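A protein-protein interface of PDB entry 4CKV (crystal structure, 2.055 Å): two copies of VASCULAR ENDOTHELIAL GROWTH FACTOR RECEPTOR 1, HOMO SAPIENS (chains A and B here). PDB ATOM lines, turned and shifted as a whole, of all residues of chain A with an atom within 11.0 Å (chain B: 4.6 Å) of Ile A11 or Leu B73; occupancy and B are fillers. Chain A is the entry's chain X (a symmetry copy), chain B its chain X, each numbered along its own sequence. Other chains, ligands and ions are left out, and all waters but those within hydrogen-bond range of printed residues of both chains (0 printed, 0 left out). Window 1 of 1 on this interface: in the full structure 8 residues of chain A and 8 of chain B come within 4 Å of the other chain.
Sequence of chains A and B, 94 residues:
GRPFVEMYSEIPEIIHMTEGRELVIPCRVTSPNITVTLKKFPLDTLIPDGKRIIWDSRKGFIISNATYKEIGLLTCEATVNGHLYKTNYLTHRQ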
ATOM      1  N   ARG A   2       6.037  39.652  13.299  1.00  0.00           N
ATOM      2  CA  ARG A   2       5.273  38.790  12.422  1.00  0.00           C
ATOM      3  C   ARG A   2       4.986  39.438  11.075  1.00  0.00           C
ATOM      4  O   ARG A   2       3.984  40.124  10.922  1.00  0.00           O
ATOM      5  CB  ARG A   2       3.960  38.416  13.095  1.00  0.00           C
ATOM      6  CG  ARG A   2       3.335  37.184  12.503  1.00  0.00           C
ATOM      7  CD  ARG A   2       2.089  36.842  13.239  1.00  0.00           C
ATOM      8  NE  ARG A   2       1.272  35.871  12.529  1.00  0.00           N
ATOM      9  CZ  ARG A   2       1.199  34.585  12.847  1.00  0.00           C
ATOM     10  NH1 ARG A   2       1.921  34.092  13.856  1.00  0.00           N
ATOM     11  NH2 ARG A   2       0.396  33.795  12.161  1.00  0.00           N
ATOM     12  N   GLU A   6      -0.623  34.916   8.228  1.00  0.00           N
ATOM     13  CA  GLU A   6      -0.688  33.507   8.615  1.00  0.00           C
ATOM     14  C   GLU A   6       0.730  32.949   8.502  1.00  0.00           C
ATOM     15  O   GLU A   6       1.349  33.065   7.459  1.00  0.00           O
ATOM     16  CB  GLU A   6      -1.618  32.716   7.671  1.00  0.00           C
ATOM     17  CG  GLU A   6      -3.119  33.004   7.820  1.00  0.00           C
ATOM     18  CD  GLU A   6      -3.541  34.364   7.254  1.00  0.00           C
ATOM     19  OE1 GLU A   6      -3.074  34.739   6.162  1.00  0.00           O
ATOM     20  OE2 GLU A   6      -4.349  35.063   7.901  1.00  0.00           O
ATOM     21  N   MET A   7       1.267  32.372   9.567  1.00  0.00           N
ATOM     22  CA  MET A   7       2.643  31.887   9.488  1.00  0.00           C
ATOM     23  C   MET A   7       2.771  30.400   9.792  1.00  0.00           C
ATOM     24  O   MET A   7       2.456  29.948  10.894  1.00  0.00           O
ATOM     25  CB  MET A   7       3.591  32.711  10.367  1.00  0.00           C
ATOM     26  CG  MET A   7       5.048  32.602   9.903  1.00  0.00           C
ATOM     27  SD  MET A   7       6.192  33.711  10.739  1.00  0.00           S
ATOM     28  CE  MET A   7       5.400  35.291  10.455  1.00  0.00           C
ATOM     29  N   TYR A   8       3.224  29.642   8.797  1.00  0.00           N
ATOM     30  CA  TYR A   8       3.390  28.195   8.961  1.00  0.00           C
ATOM     31  C   TYR A   8       4.875  27.858   8.883  1.00  0.00           C
ATOM     32  O   TYR A   8       5.377  27.435   7.844  1.00  0.00           O
ATOM     33  CB  TYR A   8       2.571  27.440   7.901  1.00  0.00           C
ATOM     34  CG  TYR A   8       1.108  27.853   7.870  1.00  0.00           C
ATOM     35  CD1 TYR A   8       0.211  27.403   8.836  1.00  0.00           C
ATOM     36  CD2 TYR A   8       0.631  28.715   6.890  1.00  0.00           C
ATOM     37  CE1 TYR A   8      -1.121  27.794   8.814  1.00  0.00           C
ATOM     38  CE2 TYR A   8      -0.696  29.105   6.858  1.00  0.00           C
ATOM     39  CZ  TYR A   8      -1.563  28.651   7.822  1.00  0.00           C
ATOM     40  OH  TYR A   8      -2.875  29.041   7.778  1.00  0.00           O
ATOM     41  N   SER A   9       5.581  28.068   9.989  1.00  0.00           N
ATOM     42  CA  SER A   9       7.033  27.917   9.996  1.00  0.00           C
ATOM     43  C   SER A   9       7.472  26.498  10.342  1.00  0.00           C
ATOM     44  O   SER A   9       8.519  26.043   9.879  1.00  0.00           O
ATOM     45  CB  SER A   9       7.669  28.902  10.977  1.00  0.00           C
ATOM     46  OG  SER A   9       7.311  28.574  12.305  1.00  0.00           O
ATOM     47  N   GLU A  10       6.670  25.804  11.142  1.00  0.00           N
ATOM     48  CA  GLU A  10       7.042  24.474  11.636  1.00  0.00           C
ATOM     49  C   GLU A  10       6.387  23.312  10.885  1.00  0.00           C
ATOM     50  O   GLU A  10       7.025  22.297  10.613  1.00  0.00           O
ATOM     51  CB  GLU A  10       6.730  24.365  13.132  1.00  0.00           C
ATOM     52  CG  GLU A  10       7.236  25.542  13.954  1.00  0.00           C
ATOM     53  CD  GLU A  10       8.753  25.600  14.025  1.00  0.00           C
ATOM     54  OE1 GLU A  10       9.381  24.537  14.218  1.00  0.00           O
ATOM     55  OE2 GLU A  10       9.316  26.711  13.887  1.00  0.00           O
ATOM     56  N   ILE A  11       5.107  23.453  10.571  1.00  0.00           N
ATOM     57  CA  ILE A  11       4.372  22.430   9.836  1.00  0.00           C
ATOM     58  C   ILE A  11       3.728  23.139   8.653  1.00  0.00           C
ATOM     59  O   ILE A  11       3.050  24.149   8.836  1.00  0.00           O
ATOM     60  CB  ILE A  11       3.285  21.780  10.715  1.00  0.00           C
ATOM     61  CG1 ILE A  11       3.929  21.045  11.902  1.00  0.00           C
ATOM     62  CG2 ILE A  11       2.408  20.830   9.885  1.00  0.00           C
ATOM     63  CD1 ILE A  11       2.922  20.533  12.939  1.00  0.00           C
ATOM     64  N   PRO A  12       3.971  22.642   7.433  1.00  0.00           N
ATOM     65  CA  PRO A  12       3.485  23.394   6.273  1.00  0.00           C
ATOM     66  C   PRO A  12       1.973  23.328   6.142  1.00  0.00           C
ATOM     67  O   PRO A  12       1.335  22.359   6.554  1.00  0.00           O
ATOM     68  CB  PRO A  12       4.134  22.672   5.077  1.00  0.00           C
ATOM     69  CG  PRO A  12       5.220  21.802   5.668  1.00  0.00           C
ATOM     70  CD  PRO A  12       4.750  21.454   7.040  1.00  0.00           C
ATOM     71  N   GLU A  13       1.410  24.367   5.551  1.00  0.00           N
ATOM     72  CA  GLU A  13      -0.003  24.379   5.216  1.00  0.00           C
ATOM     73  C   GLU A  13      -0.178  23.724   3.849  1.00  0.00           C
ATOM     74  O   GLU A  13       0.681  23.849   2.983  1.00  0.00           O
ATOM     75  CB  GLU A  13      -0.515  25.826   5.212  1.00  0.00           C
ATOM     76  CG  GLU A  13      -1.823  26.060   4.467  1.00  0.00           C
ATOM     77  CD  GLU A  13      -3.047  25.714   5.290  1.00  0.00           C
ATOM     78  OE1 GLU A  13      -2.919  24.958   6.276  1.00  0.00           O
ATOM     79  OE2 GLU A  13      -4.143  26.209   4.948  1.00  0.00           O
ATOM     80  N   ILE A  14      -1.273  23.005   3.657  1.00  0.00           N
ATOM     81  CA  ILE A  14      -1.508  22.336   2.387  1.00  0.00           C
ATOM     82  C   ILE A  14      -2.358  23.220   1.486  1.00  0.00           C
ATOM     83  O   ILE A  14      -3.352  23.790   1.927  1.00  0.00           O
ATOM     84  CB  ILE A  14      -2.224  20.982   2.573  1.00  0.00           C
ATOM     85  CG1 ILE A  14      -1.423  20.069   3.505  1.00  0.00           C
ATOM     86  CG2 ILE A  14      -2.439  20.305   1.223  1.00  0.00           C
ATOM     87  CD1 ILE A  14      -2.173  18.803   3.912  1.00  0.00           C
ATOM     88  N   ILE A  15      -1.965  23.350   0.226  1.00  0.00           N
ATOM     89  CA  ILE A  15      -2.814  24.049  -0.730  1.00  0.00           C
ATOM     90  C   ILE A  15      -2.961  23.199  -1.983  1.00  0.00           C
ATOM     91  O   ILE A  15      -2.043  22.493  -2.383  1.00  0.00           O
ATOM     92  CB  ILE A  15      -2.333  25.495  -1.030  1.00  0.00           C
ATOM     93  CG1 ILE A  15      -0.898  25.516  -1.529  1.00  0.00           C
ATOM     94  CG2 ILE A  15      -2.431  26.376   0.221  1.00  0.00           C
ATOM     95  CD1 ILE A  15      -0.267  26.917  -1.457  1.00  0.00           C
ATOM     96  N   LEU A  73       7.353  21.579  -1.899  1.00  0.00           N
ATOM     97  CA  LEU A  73       7.375  22.449  -0.739  1.00  0.00           C
ATOM     98  C   LEU A  73       7.759  23.839  -1.197  1.00  0.00           C
ATOM     99  O   LEU A  73       8.854  24.056  -1.704  1.00  0.00           O
ATOM    100  CB  LEU A  73       8.392  21.950   0.282  1.00  0.00           C
ATOM    101  CG  LEU A  73       8.640  22.870   1.479  1.00  0.00           C
ATOM    102  CD1 LEU A  73       7.380  23.019   2.342  1.00  0.00           C
ATOM    103  CD2 LEU A  73       9.808  22.325   2.298  1.00  0.00           C
ATOM    104  N   LEU A  74       6.837  24.773  -1.051  1.00  0.00           N
ATOM    105  CA  LEU A  74       7.090  26.165  -1.401  1.00  0.00           C
ATOM    106  C   LEU A  74       7.187  27.006  -0.135  1.00  0.00           C
ATOM    107  O   LEU A  74       6.384  26.846   0.786  1.00  0.00           O
ATOM    108  CB  LEU A  74       5.985  26.690  -2.317  1.00  0.00           C
ATOM    109  CG  LEU A  74       6.060  26.251  -3.779  1.00  0.00           C
ATOM    110  CD1 LEU A  74       4.679  26.270  -4.393  1.00  0.00           C
ATOM    111  CD2 LEU A  74       7.003  27.151  -4.584  1.00  0.00           C
ATOM    112  N   THR A  75       8.165  27.902  -0.092  1.00  0.00           N
ATOM    113  CA  THR A  75       8.412  28.696   1.105  1.00  0.00           C
ATOM    114  C   THR A  75       8.454  30.186   0.768  1.00  0.00           C
ATOM    115  O   THR A  75       9.153  30.598  -0.157  1.00  0.00           O
ATOM    116  CB  THR A  75       9.745  28.262   1.763  1.00  0.00           C
ATOM    117  OG1 THR A  75       9.722  26.843   2.007  1.00  0.00           O
ATOM    118  CG2 THR A  75      10.005  28.996   3.093  1.00  0.00           C
ATOM    119  N   LYS A  86      10.098  32.540   7.818  1.00  0.00           N
ATOM    120  CA  LYS A  86       9.663  31.611   6.776  1.00  0.00           C
ATOM    121  C   LYS A  86       8.260  31.088   7.040  1.00  0.00           C
ATOM    122  O   LYS A  86       7.880  30.837   8.181  1.00  0.00           O
ATOM    123  CB  LYS A  86      10.596  30.401   6.696  1.00  0.00           C
ATOM    124  CG  LYS A  86      12.063  30.732   6.550  1.00  0.00           C
ATOM    125  CD  LYS A  86      12.875  29.459   6.406  1.00  0.00           C
ATOM    126  CE  LYS A  86      14.323  29.756   6.074  1.00  0.00           C
ATOM    127  NZ  LYS A  86      15.113  28.499   5.887  1.00  0.00           N
ATOM    128  N   THR A  87       7.501  30.899   5.973  1.00  0.00           N
ATOM    129  CA  THR A  87       6.202  30.253   6.077  1.00  0.00           C
ATOM    130  C   THR A  87       6.112  29.258   4.923  1.00  0.00           C
ATOM    131  O   THR A  87       6.508  29.557   3.794  1.00  0.00           O
ATOM    132  CB  THR A  87       5.031  31.278   6.098  1.00  0.00           C
ATOM    133  OG1 THR A  87       3.780  30.592   6.210  1.00  0.00           O
ATOM    134  CG2 THR A  87       5.015  32.142   4.846  1.00  0.00           C
ATOM    135  N   ASN A  88       5.621  28.064   5.224  1.00  0.00           N
ATOM    136  CA  ASN A  88       5.765  26.925   4.325  1.00  0.00           C
ATOM    137  C   ASN A  88       4.443  26.373   3.826  1.00  0.00           C
ATOM    138  O   ASN A  88       3.473  26.270   4.576  1.00  0.00           O
ATOM    139  CB  ASN A  88       6.523  25.800   5.039  1.00  0.00           C
ATOM    140  CG  ASN A  88       7.911  26.212   5.450  1.00  0.00           C
ATOM    141  OD1 ASN A  88       8.822  26.278   4.622  1.00  0.00           O
ATOM    142  ND2 ASN A  88       8.087  26.497   6.734  1.00  0.00           N
ATOM    143  N   TYR A  89       4.421  25.994   2.557  1.00  0.00           N
ATOM    144  CA  TYR A  89       3.235  25.434   1.949  1.00  0.00           C
ATOM    145  C   TYR A  89       3.606  24.195   1.168  1.00  0.00           C
ATOM    146  O   TYR A  89       4.620  24.170   0.463  1.00  0.00           O
ATOM    147  CB  TYR A  89       2.562  26.451   1.018  1.00  0.00           C
ATOM    148  CG  TYR A  89       2.032  27.669   1.748  1.00  0.00           C
ATOM    149  CD1 TYR A  89       2.835  28.782   1.958  1.00  0.00           C
ATOM    150  CD2 TYR A  89       0.731  27.696   2.244  1.00  0.00           C
ATOM    151  CE1 TYR A  89       2.355  29.901   2.630  1.00  0.00           C
ATOM    152  CE2 TYR A  89       0.241  28.813   2.925  1.00  0.00           C
ATOM    153  CZ  TYR A  89       1.054  29.911   3.106  1.00  0.00           C
ATOM    154  OH  TYR A  89       0.567  31.021   3.772  1.00  0.00           O
ATOM    155  N   LEU A  90       2.780  23.165   1.304  1.00  0.00           N
ATOM    156  CA  LEU A  90       2.897  21.974   0.482  1.00  0.00           C
ATOM    157  C   LEU A  90       1.796  21.988  -0.570  1.00  0.00           C
ATOM    158  O   LEU A  90       0.617  21.953  -0.244  1.00  0.00           O
ATOM    159  CB  LEU A  90       2.797  20.707   1.348  1.00  0.00           C
ATOM    160  CG  LEU A  90       4.071  20.171   2.008  1.00  0.00           C
ATOM    161  CD1 LEU A  90       3.730  19.024   2.984  1.00  0.00           C
ATOM    162  CD2 LEU A  90       5.089  19.696   0.953  1.00  0.00           C
ATOM    163  N   THR A  91       2.185  22.052  -1.836  1.00  0.00           N
ATOM    164  CA  THR A  91       1.217  22.043  -2.917  1.00  0.00           C
ATOM    165  C   THR A  91       1.050  20.620  -3.431  1.00  0.00           C
ATOM    166  O   THR A  91       2.035  19.926  -3.645  1.00  0.00           O
ATOM    167  CB  THR A  91       1.682  22.928  -4.089  1.00  0.00           C
ATOM    168  OG1 THR A  91       2.996  22.537  -4.487  1.00  0.00           O
ATOM    169  CG2 THR A  91       1.721  24.395  -3.685  1.00  0.00           C
ATOM    170  N   PRO B  12       6.641  15.970   5.238  1.00  0.00           N
ATOM    171  CA  PRO B  12       5.615  14.938   5.408  1.00  0.00           C
ATOM    172  C   PRO B  12       4.925  14.597   4.099  1.00  0.00           C
ATOM    173  O   PRO B  12       4.814  15.428   3.197  1.00  0.00           O
ATOM    174  CB  PRO B  12       4.600  15.594   6.365  1.00  0.00           C
ATOM    175  CG  PRO B  12       5.308  16.795   6.948  1.00  0.00           C
ATOM    176  CD  PRO B  12       6.275  17.235   5.901  1.00  0.00           C
ATOM    177  N   LYS B  39       1.932   8.397  16.491  1.00  0.00           N
ATOM    178  CA  LYS B  39       1.751   9.632  17.254  1.00  0.00           C
ATOM    179  C   LYS B  39       0.988  10.702  16.490  1.00  0.00           C
ATOM    180  O   LYS B  39       1.069  10.782  15.262  1.00  0.00           O
ATOM    181  CB  LYS B  39       3.106  10.186  17.699  1.00  0.00           C
ATOM    182  CG  LYS B  39       3.747   9.362  18.798  1.00  0.00           C
ATOM    183  CD  LYS B  39       4.960  10.053  19.383  1.00  0.00           C
ATOM    184  CE  LYS B  39       5.565   9.218  20.500  1.00  0.00           C
ATOM    185  NZ  LYS B  39       6.869   9.773  20.967  1.00  0.00           N
ATOM    186  N   LYS B  40       0.227  11.508  17.221  1.00  0.00           N
ATOM    187  CA  LYS B  40      -0.387  12.698  16.641  1.00  0.00           C
ATOM    188  C   LYS B  40       0.161  13.929  17.346  1.00  0.00           C
ATOM    189  O   LYS B  40       0.034  14.070  18.564  1.00  0.00           O
ATOM    190  CB  LYS B  40      -1.915  12.668  16.760  1.00  0.00           C
ATOM    191  CG  LYS B  40      -2.561  14.072  16.725  1.00  0.00           C
ATOM    192  CD  LYS B  40      -3.349  14.306  15.456  1.00  0.00           C
ATOM    193  CE  LYS B  40      -3.934  15.718  15.425  1.00  0.00           C
ATOM    194  NZ  LYS B  40      -4.892  15.973  16.537  1.00  0.00           N
ATOM    195  N   PHE B  41       0.770  14.814  16.565  1.00  0.00           N
ATOM    196  CA  PHE B  41       1.395  16.015  17.093  1.00  0.00           C
ATOM    197  C   PHE B  41       0.387  16.902  17.811  1.00  0.00           C
ATOM    198  O   PHE B  41      -0.731  17.080  17.329  1.00  0.00           O
ATOM    199  CB  PHE B  41       2.031  16.798  15.946  1.00  0.00           C
ATOM    200  CG  PHE B  41       2.631  18.099  16.372  1.00  0.00           C
ATOM    201  CD1 PHE B  41       3.928  18.146  16.859  1.00  0.00           C
ATOM    202  CD2 PHE B  41       1.906  19.269  16.293  1.00  0.00           C
ATOM    203  CE1 PHE B  41       4.489  19.344  17.260  1.00  0.00           C
ATOM    204  CE2 PHE B  41       2.458  20.469  16.697  1.00  0.00           C
ATOM    205  CZ  PHE B  41       3.754  20.504  17.178  1.00  0.00           C
ATOM    206  N   GLY B  72      -4.259  16.191  11.122  1.00  0.00           N
ATOM    207  CA  GLY B  72      -3.069  16.833  11.643  1.00  0.00           C
ATOM    208  C   GLY B  72      -1.805  16.138  11.183  1.00  0.00           C
ATOM    209  O   GLY B  72      -1.790  15.483  10.146  1.00  0.00           O
ATOM    210  N   LEU B  73      -0.736  16.295  11.956  1.00  0.00           N
ATOM    211  CA  LEU B  73       0.530  15.663  11.639  1.00  0.00           C
ATOM    212  C   LEU B  73       0.613  14.359  12.402  1.00  0.00           C
ATOM    213  O   LEU B  73       0.616  14.345  13.628  1.00  0.00           O
ATOM    214  CB  LEU B  73       1.692  16.564  12.043  1.00  0.00           C
ATOM    215  CG  LEU B  73       3.086  15.948  11.922  1.00  0.00           C
ATOM    216  CD1 LEU B  73       3.433  15.630  10.460  1.00  0.00           C
ATOM    217  CD2 LEU B  73       4.111  16.899  12.537  1.00  0.00           C
ATOM    218  N   LEU B  74       0.640  13.260  11.671  1.00  0.00           N
ATOM    219  CA  LEU B  74       0.772  11.939  12.273  1.00  0.00           C
ATOM    220  C   LEU B  74       2.154  11.371  11.974  1.00  0.00           C
ATOM    221  O   LEU B  74       2.643  11.474  10.848  1.00  0.00           O
ATOM    222  CB  LEU B  74      -0.320  11.008  11.750  1.00  0.00           C
ATOM    223  CG  LEU B  74      -1.713  11.203  12.350  1.00  0.00           C
ATOM    224  CD1 LEU B  74      -2.765  10.734  11.372  1.00  0.00           C
ATOM    225  CD2 LEU B  74      -1.859  10.451  13.677  1.00  0.00           C
ATOM    226  N   THR B  75       2.778  10.771  12.980  1.00  0.00           N
ATOM    227  CA  THR B  75       4.141  10.275  12.836  1.00  0.00           C
ATOM    228  C   THR B  75       4.232   8.809  13.260  1.00  0.00           C
ATOM    229  O   THR B  75       3.765   8.441  14.338  1.00  0.00           O
ATOM    230  CB  THR B  75       5.110  11.135  13.685  1.00  0.00           C
ATOM    231  OG1 THR B  75       4.961  12.522  13.328  1.00  0.00           O
ATOM    232  CG2 THR B  75       6.582  10.721  13.488  1.00  0.00           C
ATOM    233  N   ASN B  88       6.642  10.854   8.528  1.00  0.00           N
ATOM    234  CA  ASN B  88       5.602  11.827   8.841  1.00  0.00           C
ATOM    235  C   ASN B  88       4.530  11.936   7.772  1.00  0.00           C
ATOM    236  O   ASN B  88       4.819  11.913   6.577  1.00  0.00           O
ATOM    237  CB  ASN B  88       6.235  13.209   9.037  1.00  0.00           C
ATOM    238  CG  ASN B  88       7.217  13.236  10.176  1.00  0.00           C
ATOM    239  OD1 ASN B  88       6.828  13.266  11.346  1.00  0.00           O
ATOM    240  ND2 ASN B  88       8.503  13.220   9.849  1.00  0.00           N
ATOM    241  N   TYR B  89       3.291  12.082   8.216  1.00  0.00           N
ATOM    242  CA  TYR B  89       2.168  12.216   7.314  1.00  0.00           C
ATOM    243  C   TYR B  89       1.293  13.360   7.765  1.00  0.00           C
ATOM    244  O   TYR B  89       1.028  13.525   8.960  1.00  0.00           O
ATOM    245  CB  TYR B  89       1.346  10.922   7.266  1.00  0.00           C
ATOM    246  CG  TYR B  89       2.111   9.747   6.690  1.00  0.00           C
ATOM    247  CD1 TYR B  89       2.876   8.924   7.506  1.00  0.00           C
ATOM    248  CD2 TYR B  89       2.085   9.474   5.324  1.00  0.00           C
ATOM    249  CE1 TYR B  89       3.584   7.848   6.983  1.00  0.00           C
ATOM    250  CE2 TYR B  89       2.796   8.399   4.789  1.00  0.00           C
ATOM    251  CZ  TYR B  89       3.534   7.588   5.623  1.00  0.00           C
ATOM    252  OH  TYR B  89       4.233   6.516   5.095  1.00  0.00           O
ATOM    253  N   LEU B  90       0.850  14.156   6.798  1.00  0.00           N
ATOM    254  CA  LEU B  90      -0.144  15.185   7.047  1.00  0.00           C
ATOM    255  C   LEU B  90      -1.486  14.720   6.499  1.00  0.00           C
ATOM    256  O   LEU B  90      -1.637  14.509   5.303  1.00  0.00           O
ATOM    257  CB  LEU B  90       0.275  16.511   6.388  1.00  0.00           C
ATOM    258  CG  LEU B  90       1.198  17.453   7.166  1.00  0.00           C
ATOM    259  CD1 LEU B  90       1.656  18.622   6.267  1.00  0.00           C
ATOM    260  CD2 LEU B  90       0.508  17.989   8.436  1.00  0.00           C
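The backbone NH of Phe B41 is in hydrogen-bond range of the backbone carbonyl oxygen of Leu B73 (3.0 Å). The backbone carbonyl oxygen (O) of Glu A13 sits at hydrogen-bond distance from the backbone NH (N) of Leu A90 (2.8 Å). N of Ile A15 sits at hydrogen-bond distance from O of Leu A90 (3.0 Å).
Among the printed residues, pairs that only touch across the chains: Ile A11 with Leu B90 (3.7 Å), Ile A11 with Phe B41 (3.7 Å), Pro A12 with Leu B90 (3.8 Å), Leu A90 with Pro B12 (3.8 Å), Ile A11 with Leu B73 (3.8 Å) and Leu A90 with Leu B90 (3.9 Å).
Of the printed residues of chain B, Pro A12 touches Leu B90. Glu A13 touches none of the printed residues of chain B. Leu A74 touches none of the printed residues of chain B. Of the printed residues of chain A, Pro B12 touches Leu A90 (3.8 Å). Of chain A, only Ile A11 comes within 4 Å of Phe B41. Gly B72 touches none of the printed residues of chain A. Of chain A, only Ile A11 (3.8 Å) comes within 4 Å of Leu B73. Thr B75 touches none of the printed residues of chain A. No residue of chain A comes within 4 Å of Asn B88. Of chain A, only Ile A11, Pro A12 and Leu A90 come within 4 Å of Leu B90. The nearest printed residue of chain B that does not touch Ile A11 is Pro B12 (5.8 Å). The nearest printed residue of chain B that does not touch Pro A12 is Pro B12 (4.6 Å).
Printed residues of chain A that touch a printed residue of chain B: Ile A11, Pro A12 and Leu A90. Of the 11 printed residues of chain B, 4 touch a printed residue of chain A. Printed residues of chain B that touch a printed residue of chain A: Pro B12, Phe B41, Leu B73 and Leu B90. Hydrophobic or aromatic side chains of chain B that line the printed part of chain A: Phe B41, Leu B73 and Leu B90. Among the printed residues, no Asp or Glu carboxylate lies within 4 Å of a Lys or Arg side-chain nitrogen of the other chain.
Pro A12 touches Leu B90, and with the chains exchanged Leu A90 touches Pro B12. Leu B90 touches its own counterpart, Leu A90. Of the 6 pairs that touch across the chains among the printed residues, 3 have their exchanged pair printed and touching as well.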
